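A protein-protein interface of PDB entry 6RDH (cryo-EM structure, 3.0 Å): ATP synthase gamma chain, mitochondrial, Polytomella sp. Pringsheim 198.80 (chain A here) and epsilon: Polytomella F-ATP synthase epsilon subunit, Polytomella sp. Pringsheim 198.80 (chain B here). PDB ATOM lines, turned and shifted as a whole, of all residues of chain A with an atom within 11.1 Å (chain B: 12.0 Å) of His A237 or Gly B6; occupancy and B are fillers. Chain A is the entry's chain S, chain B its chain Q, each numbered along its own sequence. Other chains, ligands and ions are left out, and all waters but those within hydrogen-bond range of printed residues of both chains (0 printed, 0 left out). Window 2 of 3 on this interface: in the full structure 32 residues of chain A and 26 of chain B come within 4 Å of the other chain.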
ATOM      1  N   TYR A 231     -15.850  15.856 -25.686  1.00  0.00           N
ATOM      2  CA  TYR A 231     -14.955  16.196 -26.781  1.00  0.00           C
ATOM      3  C   TYR A 231     -13.505  16.023 -26.369  1.00  0.00           C
ATOM      4  O   TYR A 231     -13.078  16.552 -25.341  1.00  0.00           O
ATOM      5  CB  TYR A 231     -15.187  17.633 -27.239  1.00  0.00           C
ATOM      6  CG  TYR A 231     -16.523  17.853 -27.889  1.00  0.00           C
ATOM      7  CD1 TYR A 231     -16.683  17.686 -29.255  1.00  0.00           C
ATOM      8  CD2 TYR A 231     -17.621  18.223 -27.141  1.00  0.00           C
ATOM      9  CE1 TYR A 231     -17.897  17.882 -29.851  1.00  0.00           C
ATOM     10  CE2 TYR A 231     -18.837  18.421 -27.726  1.00  0.00           C
ATOM     11  CZ  TYR A 231     -18.971  18.250 -29.082  1.00  0.00           C
ATOM     12  OH  TYR A 231     -20.194  18.453 -29.663  1.00  0.00           O
ATOM     13  N   ASP A 232     -12.753  15.304 -27.186  1.00  0.00           N
ATOM     14  CA  ASP A 232     -11.324  15.150 -26.984  1.00  0.00           C
ATOM     15  C   ASP A 232     -10.616  16.390 -27.507  1.00  0.00           C
ATOM     16  O   ASP A 232     -10.560  16.613 -28.716  1.00  0.00           O
ATOM     17  CB  ASP A 232     -10.824  13.901 -27.708  1.00  0.00           C
ATOM     18  CG  ASP A 232      -9.685  13.225 -26.989  1.00  0.00           C
ATOM     19  OD1 ASP A 232      -8.892  12.534 -27.658  1.00  0.00           O
ATOM     20  OD2 ASP A 232      -9.577  13.386 -25.758  1.00  0.00           O
ATOM     21  N   ILE A 233     -10.063  17.182 -26.602  1.00  0.00           N
ATOM     22  CA  ILE A 233      -9.438  18.440 -26.984  1.00  0.00           C
ATOM     23  C   ILE A 233      -8.070  18.137 -27.567  1.00  0.00           C
ATOM     24  O   ILE A 233      -7.259  17.442 -26.950  1.00  0.00           O
ATOM     25  CB  ILE A 233      -9.330  19.388 -25.789  1.00  0.00           C
ATOM     26  CG1 ILE A 233     -10.705  19.582 -25.180  1.00  0.00           C
ATOM     27  CG2 ILE A 233      -8.751  20.709 -26.213  1.00  0.00           C
ATOM     28  CD1 ILE A 233     -11.692  20.211 -26.110  1.00  0.00           C
ATOM     29  N   GLU A 234      -7.816  18.647 -28.762  1.00  0.00           N
ATOM     30  CA  GLU A 234      -6.591  18.367 -29.489  1.00  0.00           C
ATOM     31  C   GLU A 234      -5.822  19.653 -29.747  1.00  0.00           C
ATOM     32  O   GLU A 234      -5.272  19.860 -30.822  1.00  0.00           O
ATOM     33  CB  GLU A 234      -6.907  17.639 -30.789  1.00  0.00           C
ATOM     34  CG  GLU A 234      -5.865  16.652 -31.263  1.00  0.00           C
ATOM     35  CD  GLU A 234      -5.000  17.200 -32.373  1.00  0.00           C
ATOM     36  OE1 GLU A 234      -5.454  18.115 -33.089  1.00  0.00           O
ATOM     37  OE2 GLU A 234      -3.875  16.700 -32.547  1.00  0.00           O
ATOM     38  N   ALA A 235      -5.774  20.532 -28.765  1.00  0.00           N
ATOM     39  CA  ALA A 235      -5.033  21.775 -28.876  1.00  0.00           C
ATOM     40  C   ALA A 235      -3.695  21.630 -28.177  1.00  0.00           C
ATOM     41  O   ALA A 235      -3.392  20.604 -27.568  1.00  0.00           O
ATOM     42  CB  ALA A 235      -5.821  22.934 -28.278  1.00  0.00           C
ATOM     43  N   SER A 236      -2.887  22.682 -28.265  1.00  0.00           N
ATOM     44  CA  SER A 236      -1.595  22.667 -27.597  1.00  0.00           C
ATOM     45  C   SER A 236      -1.763  22.849 -26.096  1.00  0.00           C
ATOM     46  O   SER A 236      -1.377  21.986 -25.301  1.00  0.00           O
ATOM     47  CB  SER A 236      -0.698  23.759 -28.170  1.00  0.00           C
ATOM     48  OG  SER A 236      -1.051  25.019 -27.636  1.00  0.00           O
ATOM     49  N   HIS A 237      -2.344  23.960 -25.695  1.00  0.00           N
ATOM     50  CA  HIS A 237      -2.496  24.316 -24.296  1.00  0.00           C
ATOM     51  C   HIS A 237      -3.857  23.839 -23.790  1.00  0.00           C
ATOM     52  O   HIS A 237      -4.485  22.966 -24.390  1.00  0.00           O
ATOM     53  CB  HIS A 237      -2.253  25.810 -24.135  1.00  0.00           C
ATOM     54  CG  HIS A 237      -0.832  26.197 -24.375  1.00  0.00           C
ATOM     55  ND1 HIS A 237      -0.235  26.099 -25.612  1.00  0.00           N
ATOM     56  CD2 HIS A 237       0.118  26.661 -23.534  1.00  0.00           C
ATOM     57  CE1 HIS A 237       1.020  26.496 -25.525  1.00  0.00           C
ATOM     58  NE2 HIS A 237       1.260  26.843 -24.275  1.00  0.00           N
ATOM     59  N   GLU A 238      -4.297  24.365 -22.653  1.00  0.00           N
ATOM     60  CA  GLU A 238      -5.443  23.837 -21.933  1.00  0.00           C
ATOM     61  C   GLU A 238      -6.756  24.128 -22.648  1.00  0.00           C
ATOM     62  O   GLU A 238      -6.816  24.851 -23.642  1.00  0.00           O
ATOM     63  CB  GLU A 238      -5.479  24.407 -20.520  1.00  0.00           C
ATOM     64  CG  GLU A 238      -4.439  23.781 -19.635  1.00  0.00           C
ATOM     65  CD  GLU A 238      -4.770  22.333 -19.335  1.00  0.00           C
ATOM     66  OE1 GLU A 238      -5.961  22.026 -19.120  1.00  0.00           O
ATOM     67  OE2 GLU A 238      -3.851  21.492 -19.362  1.00  0.00           O
ATOM     68  N   ARG A 239      -7.825  23.539 -22.110  1.00  0.00           N
ATOM     69  CA  ARG A 239      -9.152  23.718 -22.681  1.00  0.00           C
ATOM     70  C   ARG A 239      -9.687  25.119 -22.440  1.00  0.00           C
ATOM     71  O   ARG A 239     -10.518  25.602 -23.217  1.00  0.00           O
ATOM     72  CB  ARG A 239     -10.115  22.688 -22.110  1.00  0.00           C
ATOM     73  CG  ARG A 239     -11.321  22.471 -22.977  1.00  0.00           C
ATOM     74  CD  ARG A 239     -12.231  21.428 -22.417  1.00  0.00           C
ATOM     75  NE  ARG A 239     -12.730  21.798 -21.108  1.00  0.00           N
ATOM     76  CZ  ARG A 239     -13.662  21.114 -20.470  1.00  0.00           C
ATOM     77  NH1 ARG A 239     -14.184  20.036 -21.033  1.00  0.00           N
ATOM     78  NH2 ARG A 239     -14.069  21.502 -19.278  1.00  0.00           N
ATOM     79  N   SER A 240      -9.237  25.782 -21.377  1.00  0.00           N
ATOM     80  CA  SER A 240      -9.606  27.176 -21.169  1.00  0.00           C
ATOM     81  C   SER A 240      -9.047  28.057 -22.273  1.00  0.00           C
ATOM     82  O   SER A 240      -9.728  28.965 -22.753  1.00  0.00           O
ATOM     83  CB  SER A 240      -9.117  27.650 -19.806  1.00  0.00           C
ATOM     84  OG  SER A 240      -7.703  27.676 -19.757  1.00  0.00           O
ATOM     85  N   ASP A 241      -7.833  27.769 -22.729  1.00  0.00           N
ATOM     86  CA  ASP A 241      -7.251  28.512 -23.834  1.00  0.00           C
ATOM     87  C   ASP A 241      -7.906  28.190 -25.166  1.00  0.00           C
ATOM     88  O   ASP A 241      -8.070  29.097 -25.988  1.00  0.00           O
ATOM     89  CB  ASP A 241      -5.754  28.239 -23.917  1.00  0.00           C
ATOM     90  CG  ASP A 241      -5.051  28.475 -22.602  1.00  0.00           C
ATOM     91  OD1 ASP A 241      -4.384  27.548 -22.101  1.00  0.00           O
ATOM     92  OD2 ASP A 241      -5.165  29.595 -22.064  1.00  0.00           O
ATOM     93  N   VAL A 242      -8.311  26.940 -25.392  1.00  0.00           N
ATOM     94  CA  VAL A 242      -8.946  26.622 -26.664  1.00  0.00           C
ATOM     95  C   VAL A 242     -10.360  27.180 -26.699  1.00  0.00           C
ATOM     96  O   VAL A 242     -10.835  27.603 -27.750  1.00  0.00           O
ATOM     97  CB  VAL A 242      -8.893  25.104 -26.960  1.00  0.00           C
ATOM     98  CG1 VAL A 242      -9.956  24.309 -26.250  1.00  0.00           C
ATOM     99  CG2 VAL A 242      -9.013  24.859 -28.410  1.00  0.00           C
ATOM    100  N   LEU A 243     -11.023  27.290 -25.546  1.00  0.00           N
ATOM    101  CA  LEU A 243     -12.323  27.944 -25.513  1.00  0.00           C
ATOM    102  C   LEU A 243     -12.189  29.454 -25.606  1.00  0.00           C
ATOM    103  O   LEU A 243     -13.065  30.116 -26.167  1.00  0.00           O
ATOM    104  CB  LEU A 243     -13.072  27.550 -24.250  1.00  0.00           C
ATOM    105  CG  LEU A 243     -14.177  26.515 -24.409  1.00  0.00           C
ATOM    106  CD1 LEU A 243     -13.631  25.190 -24.839  1.00  0.00           C
ATOM    107  CD2 LEU A 243     -14.888  26.371 -23.098  1.00  0.00           C
ATOM    108  N   ARG A 244     -11.103  30.010 -25.072  1.00  0.00           N
ATOM    109  CA  ARG A 244     -10.843  31.435 -25.204  1.00  0.00           C
ATOM    110  C   ARG A 244     -10.563  31.808 -26.653  1.00  0.00           C
ATOM    111  O   ARG A 244     -10.964  32.880 -27.108  1.00  0.00           O
ATOM    112  CB  ARG A 244      -9.679  31.819 -24.289  1.00  0.00           C
ATOM    113  CG  ARG A 244      -9.190  33.238 -24.397  1.00  0.00           C
ATOM    114  CD  ARG A 244     -10.226  34.208 -23.898  1.00  0.00           C
ATOM    115  NE  ARG A 244     -10.389  34.141 -22.455  1.00  0.00           N
ATOM    116  CZ  ARG A 244     -11.141  34.982 -21.753  1.00  0.00           C
ATOM    117  NH1 ARG A 244     -11.241  34.853 -20.437  1.00  0.00           N
ATOM    118  NH2 ARG A 244     -11.800  35.950 -22.371  1.00  0.00           N
ATOM    119  N   ASP A 245      -9.900  30.930 -27.402  1.00  0.00           N
ATOM    120  CA  ASP A 245      -9.730  31.172 -28.831  1.00  0.00           C
ATOM    121  C   ASP A 245     -11.023  30.931 -29.597  1.00  0.00           C
ATOM    122  O   ASP A 245     -11.356  31.676 -30.528  1.00  0.00           O
ATOM    123  CB  ASP A 245      -8.624  30.283 -29.385  1.00  0.00           C
ATOM    124  CG  ASP A 245      -7.304  30.496 -28.685  1.00  0.00           C
ATOM    125  OD1 ASP A 245      -6.322  29.817 -29.042  1.00  0.00           O
ATOM    126  OD2 ASP A 245      -7.245  31.338 -27.767  1.00  0.00           O
ATOM    127  N   ALA B   3       3.084  37.701 -19.213  1.00  0.00           N
ATOM    128  CA  ALA B   3       1.988  37.779 -18.249  1.00  0.00           C
ATOM    129  C   ALA B   3       0.723  36.940 -18.578  1.00  0.00           C
ATOM    130  O   ALA B   3       0.106  36.428 -17.645  1.00  0.00           O
ATOM    131  CB  ALA B   3       1.604  39.252 -18.014  1.00  0.00           C
ATOM    132  N   PRO B   4       0.312  36.779 -19.845  1.00  0.00           N
ATOM    133  CA  PRO B   4      -0.670  35.734 -20.137  1.00  0.00           C
ATOM    134  C   PRO B   4      -0.010  34.378 -20.341  1.00  0.00           C
ATOM    135  O   PRO B   4       1.157  34.268 -20.718  1.00  0.00           O
ATOM    136  CB  PRO B   4      -1.334  36.215 -21.437  1.00  0.00           C
ATOM    137  CG  PRO B   4      -0.942  37.625 -21.583  1.00  0.00           C
ATOM    138  CD  PRO B   4       0.420  37.676 -21.013  1.00  0.00           C
ATOM    139  N   SER B   5      -0.797  33.334 -20.094  1.00  0.00           N
ATOM    140  CA  SER B   5      -0.316  31.956 -20.150  1.00  0.00           C
ATOM    141  C   SER B   5      -1.207  31.172 -21.103  1.00  0.00           C
ATOM    142  O   SER B   5      -2.331  30.807 -20.753  1.00  0.00           O
ATOM    143  CB  SER B   5      -0.316  31.322 -18.768  1.00  0.00           C
ATOM    144  OG  SER B   5      -1.638  31.166 -18.292  1.00  0.00           O
ATOM    145  N   GLY B   6      -0.701  30.905 -22.295  1.00  0.00           N
ATOM    146  CA  GLY B   6      -1.420  30.115 -23.259  1.00  0.00           C
ATOM    147  C   GLY B   6      -0.564  29.860 -24.476  1.00  0.00           C
ATOM    148  O   GLY B   6       0.648  29.664 -24.375  1.00  0.00           O
ATOM    149  N   PRO B   7      -1.177  29.865 -25.653  1.00  0.00           N
ATOM    150  CA  PRO B   7      -0.408  29.724 -26.890  1.00  0.00           C
ATOM    151  C   PRO B   7       0.401  30.977 -27.167  1.00  0.00           C
ATOM    152  O   PRO B   7       0.208  32.015 -26.543  1.00  0.00           O
ATOM    153  CB  PRO B   7      -1.483  29.503 -27.947  1.00  0.00           C
ATOM    154  CG  PRO B   7      -2.706  29.112 -27.181  1.00  0.00           C
ATOM    155  CD  PRO B   7      -2.623  29.844 -25.904  1.00  0.00           C
ATOM    156  N   PHE B   8       1.309  30.870 -28.142  1.00  0.00           N
ATOM    157  CA  PHE B   8       2.335  31.893 -28.326  1.00  0.00           C
ATOM    158  C   PHE B   8       1.760  33.217 -28.806  1.00  0.00           C
ATOM    159  O   PHE B   8       2.356  34.270 -28.563  1.00  0.00           O
ATOM    160  CB  PHE B   8       3.413  31.399 -29.291  1.00  0.00           C
ATOM    161  CG  PHE B   8       2.950  31.225 -30.709  1.00  0.00           C
ATOM    162  CD1 PHE B   8       3.182  32.208 -31.656  1.00  0.00           C
ATOM    163  CD2 PHE B   8       2.331  30.058 -31.108  1.00  0.00           C
ATOM    164  CE1 PHE B   8       2.768  32.046 -32.954  1.00  0.00           C
ATOM    165  CE2 PHE B   8       1.920  29.889 -32.409  1.00  0.00           C
ATOM    166  CZ  PHE B   8       2.143  30.884 -33.331  1.00  0.00           C
ATOM    167  N   TYR B   9       0.619  33.192 -29.489  1.00  0.00           N
ATOM    168  CA  TYR B   9      -0.051  34.444 -29.803  1.00  0.00           C
ATOM    169  C   TYR B   9      -0.684  35.051 -28.563  1.00  0.00           C
ATOM    170  O   TYR B   9      -0.702  36.274 -28.415  1.00  0.00           O
ATOM    171  CB  TYR B   9      -1.097  34.233 -30.894  1.00  0.00           C
ATOM    172  CG  TYR B   9      -1.975  33.021 -30.720  1.00  0.00           C
ATOM    173  CD1 TYR B   9      -1.660  31.822 -31.334  1.00  0.00           C
ATOM    174  CD2 TYR B   9      -3.136  33.086 -29.969  1.00  0.00           C
ATOM    175  CE1 TYR B   9      -2.460  30.722 -31.186  1.00  0.00           C
ATOM    176  CE2 TYR B   9      -3.940  31.989 -29.816  1.00  0.00           C
ATOM    177  CZ  TYR B   9      -3.598  30.813 -30.426  1.00  0.00           C
ATOM    178  OH  TYR B   9      -4.398  29.711 -30.279  1.00  0.00           O
ATOM    179  N   ARG B  10      -1.180  34.218 -27.652  1.00  0.00           N
ATOM    180  CA  ARG B  10      -1.815  34.727 -26.446  1.00  0.00           C
ATOM    181  C   ARG B  10      -0.795  35.294 -25.473  1.00  0.00           C
ATOM    182  O   ARG B  10      -1.098  36.249 -24.752  1.00  0.00           O
ATOM    183  CB  ARG B  10      -2.624  33.617 -25.787  1.00  0.00           C
ATOM    184  CG  ARG B  10      -3.578  34.084 -24.732  1.00  0.00           C
ATOM    185  CD  ARG B  10      -4.691  34.898 -25.344  1.00  0.00           C
ATOM    186  NE  ARG B  10      -5.486  34.123 -26.286  1.00  0.00           N
ATOM    187  CZ  ARG B  10      -6.656  34.527 -26.767  1.00  0.00           C
ATOM    188  NH1 ARG B  10      -7.159  35.690 -26.387  1.00  0.00           N
ATOM    189  NH2 ARG B  10      -7.324  33.768 -27.617  1.00  0.00           N
ATOM    190  N   VAL B  11       0.412  34.722 -25.437  1.00  0.00           N
ATOM    191  CA  VAL B  11       1.472  35.258 -24.589  1.00  0.00           C
ATOM    192  C   VAL B  11       1.927  36.618 -25.092  1.00  0.00           C
ATOM    193  O   VAL B  11       2.191  37.526 -24.296  1.00  0.00           O
ATOM    194  CB  VAL B  11       2.647  34.266 -24.503  1.00  0.00           C
ATOM    195  CG1 VAL B  11       3.657  34.724 -23.474  1.00  0.00           C
ATOM    196  CG2 VAL B  11       2.146  32.905 -24.107  1.00  0.00           C
ATOM    197  N   ALA B  12       1.978  36.805 -26.405  1.00  0.00           N
ATOM    198  CA  ALA B  12       2.402  38.074 -26.979  1.00  0.00           C
ATOM    199  C   ALA B  12       1.291  39.113 -27.032  1.00  0.00           C
ATOM    200  O   ALA B  12       1.414  40.079 -27.790  1.00  0.00           O
ATOM    201  CB  ALA B  12       2.961  37.852 -28.383  1.00  0.00           C
ATOM    202  N   GLY B  13       0.208  38.939 -26.272  1.00  0.00           N
ATOM    203  CA  GLY B  13      -0.885  39.884 -26.243  1.00  0.00           C
ATOM    204  C   GLY B  13      -1.836  39.807 -27.413  1.00  0.00           C
ATOM    205  O   GLY B  13      -2.875  40.475 -27.388  1.00  0.00           O
ATOM    206  N   MET B  14      -1.525  39.015 -28.429  1.00  0.00           N
ATOM    207  CA  MET B  14      -2.339  38.943 -29.627  1.00  0.00           C
ATOM    208  C   MET B  14      -3.565  38.080 -29.372  1.00  0.00           C
ATOM    209  O   MET B  14      -3.498  37.074 -28.667  1.00  0.00           O
ATOM    210  CB  MET B  14      -1.508  38.373 -30.774  1.00  0.00           C
ATOM    211  CG  MET B  14      -2.099  38.537 -32.136  1.00  0.00           C
ATOM    212  SD  MET B  14      -1.038  37.782 -33.365  1.00  0.00           S
ATOM    213  CE  MET B  14       0.491  38.599 -33.000  1.00  0.00           C
ATOM    214  N   SER B  15      -4.697  38.490 -29.933  1.00  0.00           N
ATOM    215  CA  SER B  15      -5.898  37.683 -29.844  1.00  0.00           C
ATOM    216  C   SER B  15      -5.796  36.507 -30.803  1.00  0.00           C
ATOM    217  O   SER B  15      -4.882  36.421 -31.624  1.00  0.00           O
ATOM    218  CB  SER B  15      -7.136  38.516 -30.164  1.00  0.00           C
ATOM    219  OG  SER B  15      -7.096  39.768 -29.505  1.00  0.00           O
ATOM    220  N   TYR B  16      -6.747  35.582 -30.696  1.00  0.00           N
ATOM    221  CA  TYR B  16      -6.764  34.493 -31.661  1.00  0.00           C
ATOM    222  C   TYR B  16      -7.240  34.979 -33.017  1.00  0.00           C
ATOM    223  O   TYR B  16      -6.762  34.504 -34.051  1.00  0.00           O
ATOM    224  CB  TYR B  16      -7.643  33.347 -31.187  1.00  0.00           C
ATOM    225  CG  TYR B  16      -7.759  32.285 -32.241  1.00  0.00           C
ATOM    226  CD1 TYR B  16      -6.656  31.541 -32.613  1.00  0.00           C
ATOM    227  CD2 TYR B  16      -8.949  32.066 -32.906  1.00  0.00           C
ATOM    228  CE1 TYR B  16      -6.743  30.587 -33.589  1.00  0.00           C
ATOM    229  CE2 TYR B  16      -9.042  31.120 -33.887  1.00  0.00           C
ATOM    230  CZ  TYR B  16      -7.937  30.383 -34.220  1.00  0.00           C
ATOM    231  OH  TYR B  16      -8.032  29.431 -35.197  1.00  0.00           O
ATOM    232  N   TYR B  19      -4.375  36.690 -34.826  1.00  0.00           N
ATOM    233  CA  TYR B  19      -3.386  35.700 -35.238  1.00  0.00           C
ATOM    234  C   TYR B  19      -3.861  34.918 -36.452  1.00  0.00           C
ATOM    235  O   TYR B  19      -3.123  34.759 -37.434  1.00  0.00           O
ATOM    236  CB  TYR B  19      -3.089  34.761 -34.072  1.00  0.00           C
ATOM    237  CG  TYR B  19      -2.600  33.397 -34.484  1.00  0.00           C
ATOM    238  CD1 TYR B  19      -3.433  32.286 -34.414  1.00  0.00           C
ATOM    239  CD2 TYR B  19      -1.304  33.216 -34.932  1.00  0.00           C
ATOM    240  CE1 TYR B  19      -2.992  31.048 -34.794  1.00  0.00           C
ATOM    241  CE2 TYR B  19      -0.854  31.979 -35.307  1.00  0.00           C
ATOM    242  CZ  TYR B  19      -1.702  30.900 -35.238  1.00  0.00           C
ATOM    243  OH  TYR B  19      -1.257  29.656 -35.615  1.00  0.00           O
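NE2 of His A237 lies within hydrogen-bond range of O of Gly B6, at 2.9 Å. NH2 of Arg B10 is in salt-bridge range of OD2 of Asp A245 (2.4 Å). The side-chain carboxylate of Asp A241 sits close to the backbone carbonyl oxygen of Ser B5, 3.3 Å away. OD1 of Asp A245 sits close to OH of Tyr B9 (2.3 Å).
The backbone carbonyl oxygen of Tyr B9 lies within hydrogen-bond range of the backbone NH of Met B14, 2.9 Å away. OG of Ser A236 lies within hydrogen-bond range of ND1 of His A237, 2.4 Å away. N of Glu A238 is in hydrogen-bond range of OD1 of Asp A241.
Hydrophobic or aromatic side chains of chain B that line the printed part of chain A: Tyr B9 and Tyr B16. Hydrophobic or aromatic side chains of chain A that line the printed part of chain B: His A237.
Pro B7 touches His A237 (CA to CE1, 3.8 Å). Asp A241 touches Gly B6. CG of Arg A244 touches CZ of Arg B10, at 3.7 Å. Asp A245 touches Tyr B16 (O to CD2, 3.4 Å).
His A237 touches two residues of chain B. Gly B6 touches two residues of chain A. Ala A235 touches none of the printed residues of chain B. No residue of chain B comes within 4 Å of Ser A236. No residue of chain B comes within 4 Å of Glu A238. No residue of chain B comes within 4 Å of Ser A240. Of chain B, only Ser B5 (3.3 Å) and Gly B6 (3.97 Å) come within 4 Å of Asp A241. No residue of chain A comes within 4 Å of Pro B4. Ser B5 touches just one residue of chain A: Asp A241. Printed residues of chain A within 4 Å of Tyr B16: Asp A245. Of the printed residues of chain A, Tyr B9 touches Asp A245 (2.3 Å). Of the printed residues of chain B, Asp A245 touches Tyr B9, Arg B10 and Tyr B16. Printed residues of chain B within 4 Å of Arg A244: Arg B10 (3.7 Å). The nearest residue of chain B that does not touch His A237 is Phe B8 (5.1 Å). The nearest residue of chain A that does not touch Gly B6 is Ser A236 (5.8 Å).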
